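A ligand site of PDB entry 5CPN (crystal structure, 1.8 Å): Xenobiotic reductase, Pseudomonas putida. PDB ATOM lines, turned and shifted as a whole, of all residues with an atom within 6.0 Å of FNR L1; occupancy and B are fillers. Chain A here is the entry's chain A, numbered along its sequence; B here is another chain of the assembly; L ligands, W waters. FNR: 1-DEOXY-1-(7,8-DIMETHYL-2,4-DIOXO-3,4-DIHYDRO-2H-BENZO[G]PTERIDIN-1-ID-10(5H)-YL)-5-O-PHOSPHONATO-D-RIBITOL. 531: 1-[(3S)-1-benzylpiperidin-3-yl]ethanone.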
ATOM      1  N   PRO A  22      -1.891  11.083 -31.632  1.00  0.00           N
ATOM      2  CA  PRO A  22      -0.731  11.502 -30.853  1.00  0.00           C
ATOM      3  C   PRO A  22      -1.108  11.821 -29.423  1.00  0.00           C
ATOM      4  O   PRO A  22      -2.282  11.974 -29.089  1.00  0.00           O
ATOM      5  CB  PRO A  22      -0.250  12.769 -31.578  1.00  0.00           C
ATOM      6  CG  PRO A  22      -1.554  13.386 -32.074  1.00  0.00           C
ATOM      7  CD  PRO A  22      -2.487  12.216 -32.379  1.00  0.00           C
ATOM      8  N   PRO A  23      -0.093  11.928 -28.565  1.00  0.00           N
ATOM      9  CA  PRO A  23      -0.408  12.242 -27.183  1.00  0.00           C
ATOM     10  C   PRO A  23      -1.055  13.599 -27.011  1.00  0.00           C
ATOM     11  O   PRO A  23      -0.551  14.587 -27.526  1.00  0.00           O
ATOM     12  CB  PRO A  23       0.966  12.193 -26.502  1.00  0.00           C
ATOM     13  CG  PRO A  23       1.925  12.466 -27.580  1.00  0.00           C
ATOM     14  CD  PRO A  23       1.345  11.851 -28.809  1.00  0.00           C
ATOM     15  N   MET A  24      -2.181  13.622 -26.304  1.00  0.00           N
ATOM     16  CA  MET A  24      -2.914  14.850 -25.981  1.00  0.00           C
ATOM     17  C   MET A  24      -3.345  14.901 -24.531  1.00  0.00           C
ATOM     18  O   MET A  24      -4.327  14.249 -24.157  1.00  0.00           O
ATOM     19  CB  MET A  24      -4.122  14.966 -26.863  1.00  0.00           C
ATOM     20  CG  MET A  24      -3.771  15.270 -28.293  1.00  0.00           C
ATOM     21  SD  MET A  24      -5.193  15.430 -29.392  1.00  0.00           S
ATOM     22  CE  MET A  24      -5.831  13.757 -29.269  1.00  0.00           C
ATOM     23  N   CYS A  25      -2.569  15.640 -23.721  1.00  0.00           N
ATOM     24  CA  CYS A  25      -2.922  16.000 -22.330  1.00  0.00           C
ATOM     25  C   CYS A  25      -4.386  16.345 -22.148  1.00  0.00           C
ATOM     26  O   CYS A  25      -4.952  17.146 -22.905  1.00  0.00           O
ATOM     27  CB  CYS A  25      -2.072  17.193 -21.880  1.00  0.00           C
ATOM     28  SG  CYS A  25      -0.372  16.749 -21.520  1.00  0.00           S
ATOM     29  N   GLN A  26      -4.981  15.766 -21.101  1.00  0.00           N
ATOM     30  CA  GLN A  26      -6.400  15.977 -20.771  1.00  0.00           C
ATOM     31  C   GLN A  26      -6.592  16.864 -19.562  1.00  0.00           C
ATOM     32  O   GLN A  26      -7.659  17.418 -19.354  1.00  0.00           O
ATOM     33  CB  GLN A  26      -7.093  14.637 -20.552  1.00  0.00           C
ATOM     34  CG  GLN A  26      -7.191  13.799 -21.845  1.00  0.00           C
ATOM     35  CD  GLN A  26      -7.912  14.465 -22.966  1.00  0.00           C
ATOM     36  OE1 GLN A  26      -9.152  14.568 -22.963  1.00  0.00           O
ATOM     37  NE2 GLN A  26      -7.180  14.876 -23.971  1.00  0.00           N
ATOM     38  N   TYR A  27      -5.530  17.017 -18.778  1.00  0.00           N
ATOM     39  CA  TYR A  27      -5.511  17.835 -17.576  1.00  0.00           C
ATOM     40  C   TYR A  27      -6.644  17.436 -16.644  1.00  0.00           C
ATOM     41  O   TYR A  27      -7.226  18.288 -15.968  1.00  0.00           O
ATOM     42  CB  TYR A  27      -5.613  19.337 -17.921  1.00  0.00           C
ATOM     43  CG  TYR A  27      -4.627  19.769 -18.982  1.00  0.00           C
ATOM     44  CD1 TYR A  27      -3.355  20.213 -18.630  1.00  0.00           C
ATOM     45  CD2 TYR A  27      -4.959  19.712 -20.321  1.00  0.00           C
ATOM     46  CE1 TYR A  27      -2.464  20.595 -19.598  1.00  0.00           C
ATOM     47  CE2 TYR A  27      -4.050  20.098 -21.302  1.00  0.00           C
ATOM     48  CZ  TYR A  27      -2.806  20.546 -20.931  1.00  0.00           C
ATOM     49  OH  TYR A  27      -1.881  20.927 -21.883  1.00  0.00           O
ATOM     50  N   VAL A  55      -0.978   7.413 -25.477  1.00  0.00           N
ATOM     51  CA  VAL A  55      -1.519   8.116 -24.310  1.00  0.00           C
ATOM     52  C   VAL A  55      -0.681   9.384 -24.037  1.00  0.00           C
ATOM     53  O   VAL A  55       0.557   9.406 -24.224  1.00  0.00           O
ATOM     54  CB  VAL A  55      -1.551   7.153 -23.096  1.00  0.00           C
ATOM     55  CG1 VAL A  55      -1.694   7.890 -21.771  1.00  0.00           C
ATOM     56  CG2 VAL A  55      -2.661   6.087 -23.274  1.00  0.00           C
ATOM     57  N   GLU A  56      -1.378  10.436 -23.610  1.00  0.00           N
ATOM     58  CA  GLU A  56      -0.798  11.749 -23.253  1.00  0.00           C
ATOM     59  C   GLU A  56       0.472  11.714 -22.428  1.00  0.00           C
ATOM     60  O   GLU A  56       0.718  10.765 -21.722  1.00  0.00           O
ATOM     61  CB  GLU A  56      -1.825  12.565 -22.447  1.00  0.00           C
ATOM     62  CG  GLU A  56      -2.126  11.949 -21.089  1.00  0.00           C
ATOM     63  CD  GLU A  56      -3.496  12.406 -20.486  1.00  0.00           C
ATOM     64  OE1 GLU A  56      -3.523  13.444 -19.757  1.00  0.00           O
ATOM     65  OE2 GLU A  56      -4.515  11.710 -20.714  1.00  0.00           O
ATOM     66  N   ALA A  57       1.186  12.843 -22.457  1.00  0.00           N
ATOM     67  CA  ALA A  57       2.382  13.086 -21.680  1.00  0.00           C
ATOM     68  C   ALA A  57       2.178  12.758 -20.222  1.00  0.00           C
ATOM     69  O   ALA A  57       1.385  13.387 -19.507  1.00  0.00           O
ATOM     70  CB  ALA A  57       2.833  14.544 -21.847  1.00  0.00           C
ATOM     71  N   GLN A  99       3.432   8.235 -23.909  1.00  0.00           N
ATOM     72  CA  GLN A  99       4.499   9.219 -23.945  1.00  0.00           C
ATOM     73  C   GLN A  99       4.907   9.511 -22.508  1.00  0.00           C
ATOM     74  O   GLN A  99       4.051   9.911 -21.716  1.00  0.00           O
ATOM     75  CB  GLN A  99       4.043  10.509 -24.616  1.00  0.00           C
ATOM     76  CG  GLN A  99       5.146  11.531 -24.730  1.00  0.00           C
ATOM     77  CD  GLN A  99       4.671  12.844 -25.290  1.00  0.00           C
ATOM     78  OE1 GLN A  99       3.870  13.541 -24.675  1.00  0.00           O
ATOM     79  NE2 GLN A  99       5.149  13.179 -26.491  1.00  0.00           N
ATOM     80  N   GLU A 176       7.145   6.373 -26.127  1.00  0.00           N
ATOM     81  CA  GLU A 176       7.583   7.615 -26.753  1.00  0.00           C
ATOM     82  C   GLU A 176       8.199   8.509 -25.685  1.00  0.00           C
ATOM     83  O   GLU A 176       7.497   8.914 -24.731  1.00  0.00           O
ATOM     84  CB  GLU A 176       6.426   8.334 -27.450  1.00  0.00           C
ATOM     85  CG  GLU A 176       6.851   9.586 -28.302  1.00  0.00           C
ATOM     86  CD  GLU A 176       5.640  10.265 -28.954  1.00  0.00           C
ATOM     87  OE1 GLU A 176       4.872   9.593 -29.680  1.00  0.00           O
ATOM     88  OE2 GLU A 176       5.448  11.489 -28.730  1.00  0.00           O
ATOM     89  N   HIS A 178       9.421  12.016 -24.498  1.00  0.00           N
ATOM     90  CA  HIS A 178       9.045  13.384 -24.870  1.00  0.00           C
ATOM     91  C   HIS A 178      10.285  14.281 -24.789  1.00  0.00           C
ATOM     92  O   HIS A 178      10.605  14.867 -23.739  1.00  0.00           O
ATOM     93  CB  HIS A 178       7.918  13.922 -23.972  1.00  0.00           C
ATOM     94  CG  HIS A 178       7.193  15.092 -24.547  1.00  0.00           C
ATOM     95  ND1 HIS A 178       7.630  15.752 -25.682  1.00  0.00           N
ATOM     96  CD2 HIS A 178       6.026  15.696 -24.176  1.00  0.00           C
ATOM     97  CE1 HIS A 178       6.783  16.734 -25.970  1.00  0.00           C
ATOM     98  NE2 HIS A 178       5.794  16.717 -25.077  1.00  0.00           N
ATOM     99  N   ALA A 180      10.540  16.883 -26.842  1.00  0.00           N
ATOM    100  CA  ALA A 180      10.140  18.005 -27.677  1.00  0.00           C
ATOM    101  C   ALA A 180       9.409  19.114 -26.909  1.00  0.00           C
ATOM    102  O   ALA A 180       9.223  19.038 -25.705  1.00  0.00           O
ATOM    103  CB  ALA A 180       9.261  17.504 -28.834  1.00  0.00           C
ATOM    104  N   HIS A 181       9.028  20.163 -27.638  1.00  0.00           N
ATOM    105  CA  HIS A 181       8.062  21.172 -27.176  1.00  0.00           C
ATOM    106  C   HIS A 181       8.522  21.966 -25.951  1.00  0.00           C
ATOM    107  O   HIS A 181       7.716  22.542 -25.241  1.00  0.00           O
ATOM    108  CB  HIS A 181       6.690  20.527 -26.867  1.00  0.00           C
ATOM    109  CG  HIS A 181       6.107  19.794 -28.047  1.00  0.00           C
ATOM    110  ND1 HIS A 181       5.031  18.932 -27.916  1.00  0.00           N
ATOM    111  CD2 HIS A 181       6.434  19.794 -29.355  1.00  0.00           C
ATOM    112  CE1 HIS A 181       4.739  18.427 -29.099  1.00  0.00           C
ATOM    113  NE2 HIS A 181       5.567  18.946 -29.989  1.00  0.00           N
ATOM    114  N   ARG A 231       9.832  11.811 -29.440  1.00  0.00           N
ATOM    115  CA  ARG A 231       9.406  13.016 -30.107  1.00  0.00           C
ATOM    116  C   ARG A 231      10.455  14.088 -29.821  1.00  0.00           C
ATOM    117  O   ARG A 231      10.934  14.226 -28.684  1.00  0.00           O
ATOM    118  CB  ARG A 231       7.997  13.467 -29.652  1.00  0.00           C
ATOM    119  CG  ARG A 231       7.589  14.804 -30.293  1.00  0.00           C
ATOM    120  CD  ARG A 231       6.426  14.715 -31.232  1.00  0.00           C
ATOM    121  NE  ARG A 231       5.213  15.046 -30.543  1.00  0.00           N
ATOM    122  CZ  ARG A 231       4.035  15.396 -31.087  1.00  0.00           C
ATOM    123  NH1 ARG A 231       3.800  15.597 -32.376  1.00  0.00           N
ATOM    124  NH2 ARG A 231       3.071  15.605 -30.256  1.00  0.00           N
ATOM    125  N   SER A 266       8.709  17.160 -34.628  1.00  0.00           N
ATOM    126  CA  SER A 266       7.948  18.318 -34.234  1.00  0.00           C
ATOM    127  C   SER A 266       8.739  19.621 -34.200  1.00  0.00           C
ATOM    128  O   SER A 266       9.791  19.734 -34.781  1.00  0.00           O
ATOM    129  CB  SER A 266       7.340  18.061 -32.872  1.00  0.00           C
ATOM    130  OG  SER A 266       6.193  18.885 -32.740  1.00  0.00           O
ATOM    131  N   ALA A 301       2.645  15.820 -37.199  1.00  0.00           N
ATOM    132  CA  ALA A 301       1.317  16.300 -36.859  1.00  0.00           C
ATOM    133  C   ALA A 301       1.176  17.776 -37.293  1.00  0.00           C
ATOM    134  O   ALA A 301       1.953  18.272 -38.129  1.00  0.00           O
ATOM    135  CB  ALA A 301       1.033  16.113 -35.305  1.00  0.00           C
ATOM    136  N   TRP A 302       0.179  18.464 -36.741  1.00  0.00           N
ATOM    137  CA  TRP A 302       0.050  19.914 -36.901  1.00  0.00           C
ATOM    138  C   TRP A 302      -0.540  20.277 -38.255  1.00  0.00           C
ATOM    139  O   TRP A 302       0.085  21.026 -39.012  1.00  0.00           O
ATOM    140  CB  TRP A 302       1.412  20.628 -36.748  1.00  0.00           C
ATOM    141  CG  TRP A 302       2.194  20.254 -35.505  1.00  0.00           C
ATOM    142  CD1 TRP A 302       3.290  19.449 -35.430  1.00  0.00           C
ATOM    143  CD2 TRP A 302       1.924  20.690 -34.167  1.00  0.00           C
ATOM    144  NE1 TRP A 302       3.732  19.357 -34.138  1.00  0.00           N
ATOM    145  CE2 TRP A 302       2.897  20.105 -33.336  1.00  0.00           C
ATOM    146  CE3 TRP A 302       0.955  21.511 -33.591  1.00  0.00           C
ATOM    147  CZ2 TRP A 302       2.929  20.311 -31.986  1.00  0.00           C
ATOM    148  CZ3 TRP A 302       0.999  21.726 -32.238  1.00  0.00           C
ATOM    149  CH2 TRP A 302       1.973  21.129 -31.449  1.00  0.00           C
ATOM    150  N   GLY A 303      -1.739  19.765 -38.543  1.00  0.00           N
ATOM    151  CA  GLY A 303      -2.452  20.153 -39.744  1.00  0.00           C
ATOM    152  C   GLY A 303      -2.983  19.018 -40.604  1.00  0.00           C
ATOM    153  O   GLY A 303      -3.934  19.201 -41.378  1.00  0.00           O
ATOM    154  N   PHE A 304      -2.426  17.822 -40.422  1.00  0.00           N
ATOM    155  CA  PHE A 304      -2.662  16.694 -41.343  1.00  0.00           C
ATOM    156  C   PHE A 304      -4.056  16.131 -41.158  1.00  0.00           C
ATOM    157  O   PHE A 304      -4.412  15.131 -41.762  1.00  0.00           O
ATOM    158  CB  PHE A 304      -1.631  15.562 -41.140  1.00  0.00           C
ATOM    159  CG  PHE A 304      -0.250  15.908 -41.575  1.00  0.00           C
ATOM    160  CD1 PHE A 304       0.142  15.781 -42.898  1.00  0.00           C
ATOM    161  CD2 PHE A 304       0.675  16.355 -40.645  1.00  0.00           C
ATOM    162  CE1 PHE A 304       1.420  16.102 -43.283  1.00  0.00           C
ATOM    163  CE2 PHE A 304       1.985  16.679 -41.022  1.00  0.00           C
ATOM    164  CZ  PHE A 304       2.345  16.548 -42.353  1.00  0.00           C
ATOM    165  N   GLY A 305      -4.879  16.783 -40.332  1.00  0.00           N
ATOM    166  CA  GLY A 305      -6.181  16.237 -39.990  1.00  0.00           C
ATOM    167  C   GLY A 305      -7.310  16.401 -41.000  1.00  0.00           C
ATOM    168  O   GLY A 305      -8.428  16.713 -40.654  1.00  0.00           O
ATOM    169  N   SER A 323      -0.037  11.391 -37.660  1.00  0.00           N
ATOM    170  CA  SER A 323      -0.670  11.731 -36.394  1.00  0.00           C
ATOM    171  C   SER A 323      -1.786  12.769 -36.554  1.00  0.00           C
ATOM    172  O   SER A 323      -1.598  13.847 -37.136  1.00  0.00           O
ATOM    173  CB  SER A 323       0.360  12.234 -35.404  1.00  0.00           C
ATOM    174  OG  SER A 323       1.339  11.219 -35.171  1.00  0.00           O
ATOM    175  N   VAL A 324      -2.968  12.408 -36.034  1.00  0.00           N
ATOM    176  CA  VAL A 324      -4.183  13.215 -36.146  1.00  0.00           C
ATOM    177  C   VAL A 324      -4.732  13.402 -34.749  1.00  0.00           C
ATOM    178  O   VAL A 324      -5.296  12.472 -34.177  1.00  0.00           O
ATOM    179  CB  VAL A 324      -5.224  12.538 -37.070  1.00  0.00           C
ATOM    180  CG1 VAL A 324      -6.540  13.364 -37.129  1.00  0.00           C
ATOM    181  CG2 VAL A 324      -4.641  12.300 -38.445  1.00  0.00           C
ATOM    182  N   GLY A 325      -4.550  14.603 -34.220  1.00  0.00           N
ATOM    183  CA  GLY A 325      -4.929  14.898 -32.850  1.00  0.00           C
ATOM    184  C   GLY A 325      -6.299  15.554 -32.693  1.00  0.00           C
ATOM    185  O   GLY A 325      -7.288  14.900 -32.354  1.00  0.00           O
ATOM    186  N   ARG A 326      -6.342  16.863 -32.867  1.00  0.00           N
ATOM    187  CA  ARG A 326      -7.544  17.615 -32.592  1.00  0.00           C
ATOM    188  C   ARG A 326      -8.762  17.085 -33.342  1.00  0.00           C
ATOM    189  O   ARG A 326      -9.868  17.123 -32.794  1.00  0.00           O
ATOM    190  CB  ARG A 326      -7.311  19.090 -32.884  1.00  0.00           C
ATOM    191  CG  ARG A 326      -6.499  19.765 -31.779  1.00  0.00           C
ATOM    192  CD  ARG A 326      -6.066  21.170 -32.136  1.00  0.00           C
ATOM    193  NE  ARG A 326      -5.073  21.137 -33.209  1.00  0.00           N
ATOM    194  CZ  ARG A 326      -4.388  22.196 -33.646  1.00  0.00           C
ATOM    195  NH1 ARG A 326      -4.544  23.370 -33.072  1.00  0.00           N
ATOM    196  NH2 ARG A 326      -3.540  22.048 -34.666  1.00  0.00           N
ATOM    197  N   ALA A 327      -8.603  16.535 -34.551  1.00  0.00           N
ATOM    198  CA  ALA A 327      -9.784  16.029 -35.270  1.00  0.00           C
ATOM    199  C   ALA A 327     -10.432  14.842 -34.528  1.00  0.00           C
ATOM    200  O   ALA A 327     -11.626  14.572 -34.713  1.00  0.00           O
ATOM    201  CB  ALA A 327      -9.435  15.620 -36.677  1.00  0.00           C
ATOM    202  N   LEU A 329     -10.478  14.783 -31.133  1.00  0.00           N
ATOM    203  CA  LEU A 329     -11.176  15.428 -30.030  1.00  0.00           C
ATOM    204  C   LEU A 329     -12.591  15.786 -30.491  1.00  0.00           C
ATOM    205  O   LEU A 329     -13.582  15.568 -29.796  1.00  0.00           O
ATOM    206  CB  LEU A 329     -10.390  16.656 -29.548  1.00  0.00           C
ATOM    207  CG  LEU A 329      -8.963  16.385 -29.039  1.00  0.00           C
ATOM    208  CD1 LEU A 329      -8.384  17.618 -28.412  1.00  0.00           C
ATOM    209  CD2 LEU A 329      -8.910  15.222 -28.047  1.00  0.00           C
ATOM    210  N   PRO B 354     -11.749  19.763 -21.764  1.00  0.00           N
ATOM    211  CA  PRO B 354     -10.490  19.220 -22.350  1.00  0.00           C
ATOM    212  C   PRO B 354     -10.539  19.133 -23.850  1.00  0.00           C
ATOM    213  O   PRO B 354      -9.485  19.043 -24.500  1.00  0.00           O
ATOM    214  CB  PRO B 354     -10.377  17.818 -21.751  1.00  0.00           C
ATOM    215  CG  PRO B 354     -11.189  17.881 -20.483  1.00  0.00           C
ATOM    216  CD  PRO B 354     -12.363  18.818 -20.819  1.00  0.00           C
ATOM    217  N   TRP B 358      -9.558  23.493 -26.845  1.00  0.00           N
ATOM    218  CA  TRP B 358      -8.700  23.332 -27.967  1.00  0.00           C
ATOM    219  C   TRP B 358      -9.439  23.506 -29.275  1.00  0.00           C
ATOM    220  O   TRP B 358      -8.846  23.926 -30.261  1.00  0.00           O
ATOM    221  CB  TRP B 358      -8.030  21.957 -27.862  1.00  0.00           C
ATOM    222  CG  TRP B 358      -7.189  21.873 -26.615  1.00  0.00           C
ATOM    223  CD1 TRP B 358      -7.520  21.278 -25.415  1.00  0.00           C
ATOM    224  CD2 TRP B 358      -5.921  22.489 -26.408  1.00  0.00           C
ATOM    225  NE1 TRP B 358      -6.503  21.458 -24.502  1.00  0.00           N
ATOM    226  CE2 TRP B 358      -5.502  22.187 -25.105  1.00  0.00           C
ATOM    227  CE3 TRP B 358      -5.066  23.224 -27.237  1.00  0.00           C
ATOM    228  CZ2 TRP B 358      -4.273  22.621 -24.599  1.00  0.00           C
ATOM    229  CZ3 TRP B 358      -3.835  23.631 -26.724  1.00  0.00           C
ATOM    230  CH2 TRP B 358      -3.469  23.340 -25.428  1.00  0.00           C
HETATM  231  C9A FNR L   1      -1.289  18.483 -27.560  1.00  0.00           C
HETATM  232  N10 FNR L   1      -0.035  17.925 -28.118  1.00  0.00           N
HETATM  233  CAA FNR L   1       0.844  17.058 -27.316  1.00  0.00           C
HETATM  234  N1  FNR L   1       2.125  16.880 -27.672  1.00  0.00           N
HETATM  235  C2  FNR L   1       2.837  15.961 -26.986  1.00  0.00           C
HETATM  236  O2  FNR L   1       3.913  15.617 -27.390  1.00  0.00           O
HETATM  237  N3  FNR L   1       2.340  15.435 -25.810  1.00  0.00           N
HETATM  238  C4  FNR L   1       1.168  15.783 -25.328  1.00  0.00           C
HETATM  239  O4  FNR L   1       0.755  15.279 -24.294  1.00  0.00           O
HETATM  240  C4A FNR L   1       0.474  16.756 -26.033  1.00  0.00           C
HETATM  241  N5  FNR L   1      -0.738  17.331 -25.473  1.00  0.00           N
HETATM  242  C5A FNR L   1      -1.633  18.197 -26.250  1.00  0.00           C
HETATM  243  C6  FNR L   1      -2.939  18.305 -25.801  1.00  0.00           C
HETATM  244  C7  FNR L   1      -3.900  18.793 -26.666  1.00  0.00           C
HETATM  245  C7M FNR L   1      -5.311  18.850 -26.122  1.00  0.00           C
HETATM  246  C8  FNR L   1      -3.556  19.193 -27.934  1.00  0.00           C
HETATM  247  C8M FNR L   1      -4.649  19.706 -28.855  1.00  0.00           C
HETATM  248  C9  FNR L   1      -2.269  19.100 -28.383  1.00  0.00           C
HETATM  249  C1' FNR L   1       0.360  18.165 -29.523  1.00  0.00           C
HETATM  250  C2' FNR L   1      -0.379  17.117 -30.365  1.00  0.00           C
HETATM  251  O2' FNR L   1       0.220  15.874 -30.066  1.00  0.00           O
HETATM  252  C3' FNR L   1      -0.338  17.426 -31.875  1.00  0.00           C
HETATM  253  O3' FNR L   1       1.047  17.537 -32.260  1.00  0.00           O
HETATM  254  C4' FNR L   1      -1.092  18.711 -32.192  1.00  0.00           C
HETATM  255  O4' FNR L   1      -2.398  18.649 -31.665  1.00  0.00           O
HETATM  256  C5' FNR L   1      -1.195  18.980 -33.700  1.00  0.00           C
HETATM  257  O5' FNR L   1      -1.781  17.915 -34.381  1.00  0.00           O
HETATM  258  P   FNR L   1      -3.282  18.174 -34.954  1.00  0.00           P
HETATM  259  O1P FNR L   1      -3.222  19.382 -35.846  1.00  0.00           O
HETATM  260  O2P FNR L   1      -4.122  18.431 -33.697  1.00  0.00           O
HETATM  261  O3P FNR L   1      -3.746  16.948 -35.726  1.00  0.00           O
HETATM  262  C1  531 L   2       1.525  22.391 -27.667  1.00  0.00           C
HETATM  263  C2  531 L   2       0.410  22.887 -28.593  1.00  0.00           C
HETATM  264  C3  531 L   2       0.476  24.082 -29.132  1.00  0.00           C
HETATM  265  C4  531 L   2      -0.650  24.570 -30.062  1.00  0.00           C
HETATM  266  C5  531 L   2      -1.679  23.782 -30.329  1.00  0.00           C
HETATM  267  C6  531 L   2      -1.762  22.399 -29.696  1.00  0.00           C
HETATM  268  C7  531 L   2      -0.792  21.981 -28.897  1.00  0.00           C
HETATM  269  N8  531 L   2       1.094  21.563 -26.687  1.00  0.00           N
HETATM  270  C9  531 L   2       2.085  20.920 -26.068  1.00  0.00           C
HETATM  271  C10 531 L   2       1.572  19.791 -25.212  1.00  0.00           C
HETATM  272  C11 531 L   2       0.853  20.383 -24.007  1.00  0.00           C
HETATM  273  C12 531 L   2      -0.090  21.493 -24.483  1.00  0.00           C
HETATM  274  C13 531 L   2       0.303  22.189 -25.800  1.00  0.00           C
HETATM  275  C14 531 L   2       2.586  18.670 -24.836  1.00  0.00           C
HETATM  276  O15 531 L   2       3.728  18.628 -25.615  1.00  0.00           O
HETATM  277  C16 531 L   2       2.808  18.407 -23.347  1.00  0.00           C
HETATM  278  O   HOH W   1      -6.358  16.920 -36.368  1.00  0.00           O
HETATM  279  O   HOH W   2      -2.126  16.277 -37.792  1.00  0.00           O
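A nitrogen (N3) of FNR L1 sits at hydrogen-bond distance from the side-chain amide oxygen (OE1) of Gln 99 (2.7 Å). An oxygen (O15) of 531 L2 lies within hydrogen-bond range of a ring nitrogen (ND1) of His 181, at 2.7 Å. N of Gly 325 sits at hydrogen-bond distance from O3P of FNR L1. O5' of FNR L1 is in hydrogen-bond range of N of Trp 302, at 3.1 Å. The backbone NH of Gly 303 is in hydrogen-bond range of an oxygen (O1P) of FNR L1 (3.1 Å). The guanidinium group (NE) of Arg 326 lies within salt-bridge range of an oxygen (O2P) of FNR L1 (2.9 Å). SG of Cys 25 is in hydrogen-bond range of O4 of FNR L1. The backbone NH (N) of Cys 25 sits at hydrogen-bond distance from an oxygen (O4) of FNR L1 (3.4 Å). A ring nitrogen (NE2) of His 178 is in hydrogen-bond range of an oxygen (O15) of 531 L2, at 2.9 Å. NH2 of Arg 231 is in hydrogen-bond range of O2' of FNR L1 (2.9 Å). The backbone NH (N) of Arg 326 is in hydrogen-bond range of an oxygen (O2P) of FNR L1, 2.8 Å away. O4 of FNR L1 sits at hydrogen-bond distance from N of Ala 57 (3.1 Å). NE2 of His 178 lies within hydrogen-bond range of O2 of FNR L1 (3.2 Å). The backbone carbonyl oxygen of Pro 23 sits close to an oxygen (O2') of FNR L1 (2.9 Å).
A nitrogen (N1) of FNR L1 sits close to an oxygen (O15) of 531 L2 (3.1 Å).
The backbone NH of Gln 99 sits at hydrogen-bond distance from the backbone carbonyl oxygen of Val 55 (3.1 Å). The indole nitrogen of Trp 302 is in hydrogen-bond range of the side-chain hydroxyl of Ser 266 (2.9 Å). The guanidinium group (NE) of Arg 231 lies within salt-bridge range of the side-chain carboxylate (OE2) of Glu 176 (3.999 Å). A ring nitrogen (NE2) of His 181 lies within hydrogen-bond range of the side-chain hydroxyl (OG) of Ser 266. The side-chain carboxylate of Glu 56 is in hydrogen-bond range of the backbone NH of Gln 26 (3.1 Å). ND1 of His 178 sits close to N of Ala 180 (3.3 Å). The side-chain amide nitrogen (NE2) of Gln 99 is in hydrogen-bond range of the side-chain carboxylate (OE2) of Glu 176, at 2.8 Å. The backbone carbonyl oxygen (O) of Met 24 lies within hydrogen-bond range of the side-chain amide nitrogen (NE2) of Gln 26, 2.9 Å away.
CB of Pro 22 touches O2' of FNR L1, at 3.5 Å. CA of Met 24 touches N5 of FNR L1, 3.3 Å away. CA of Glu 56 touches O4 of FNR L1, at 3.99 Å. His 181 touches FNR L1 (CE1 to N1, 3.4 Å). Ala 301 touches FNR L1. Val 324 touches FNR L1 (CA to O3P, 3.8 Å). NE1 of Trp 358 of chain B touches C7M of FNR L1, at 3.3 Å. Hydrophobic or aromatic side chains that line FNR L1: Pro 22, Pro 23, Met 24, Ala 57, His 178, His 181, Ala 301, Trp 302 and Trp 358 of chain B. 17 residues have an atom within 4 Å of FNR L1: Pro 22, Pro 23, Met 24, Cys 25, Glu 56, Ala 57, Gln 99, His 178, His 181, Arg 231, Ala 301, Trp 302, Gly 303, Val 324, Gly 325, Arg 326 and Trp 358 of chain B.
Water W1 lies within hydrogen-bond range of an oxygen (O3P) of FNR L1 (2.7 Å) and the backbone NH (N) of Ala 327 (2.9 Å). Water W2 lies within hydrogen-bond range of the backbone carbonyl oxygen (O) of Ser 323 (2.6 Å), an oxygen (O3P) of FNR L1 (2.7 Å), the backbone NH (N) of Phe 304 (3.1 Å) and the backbone NH (N) of Trp 302 (3.3 Å).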
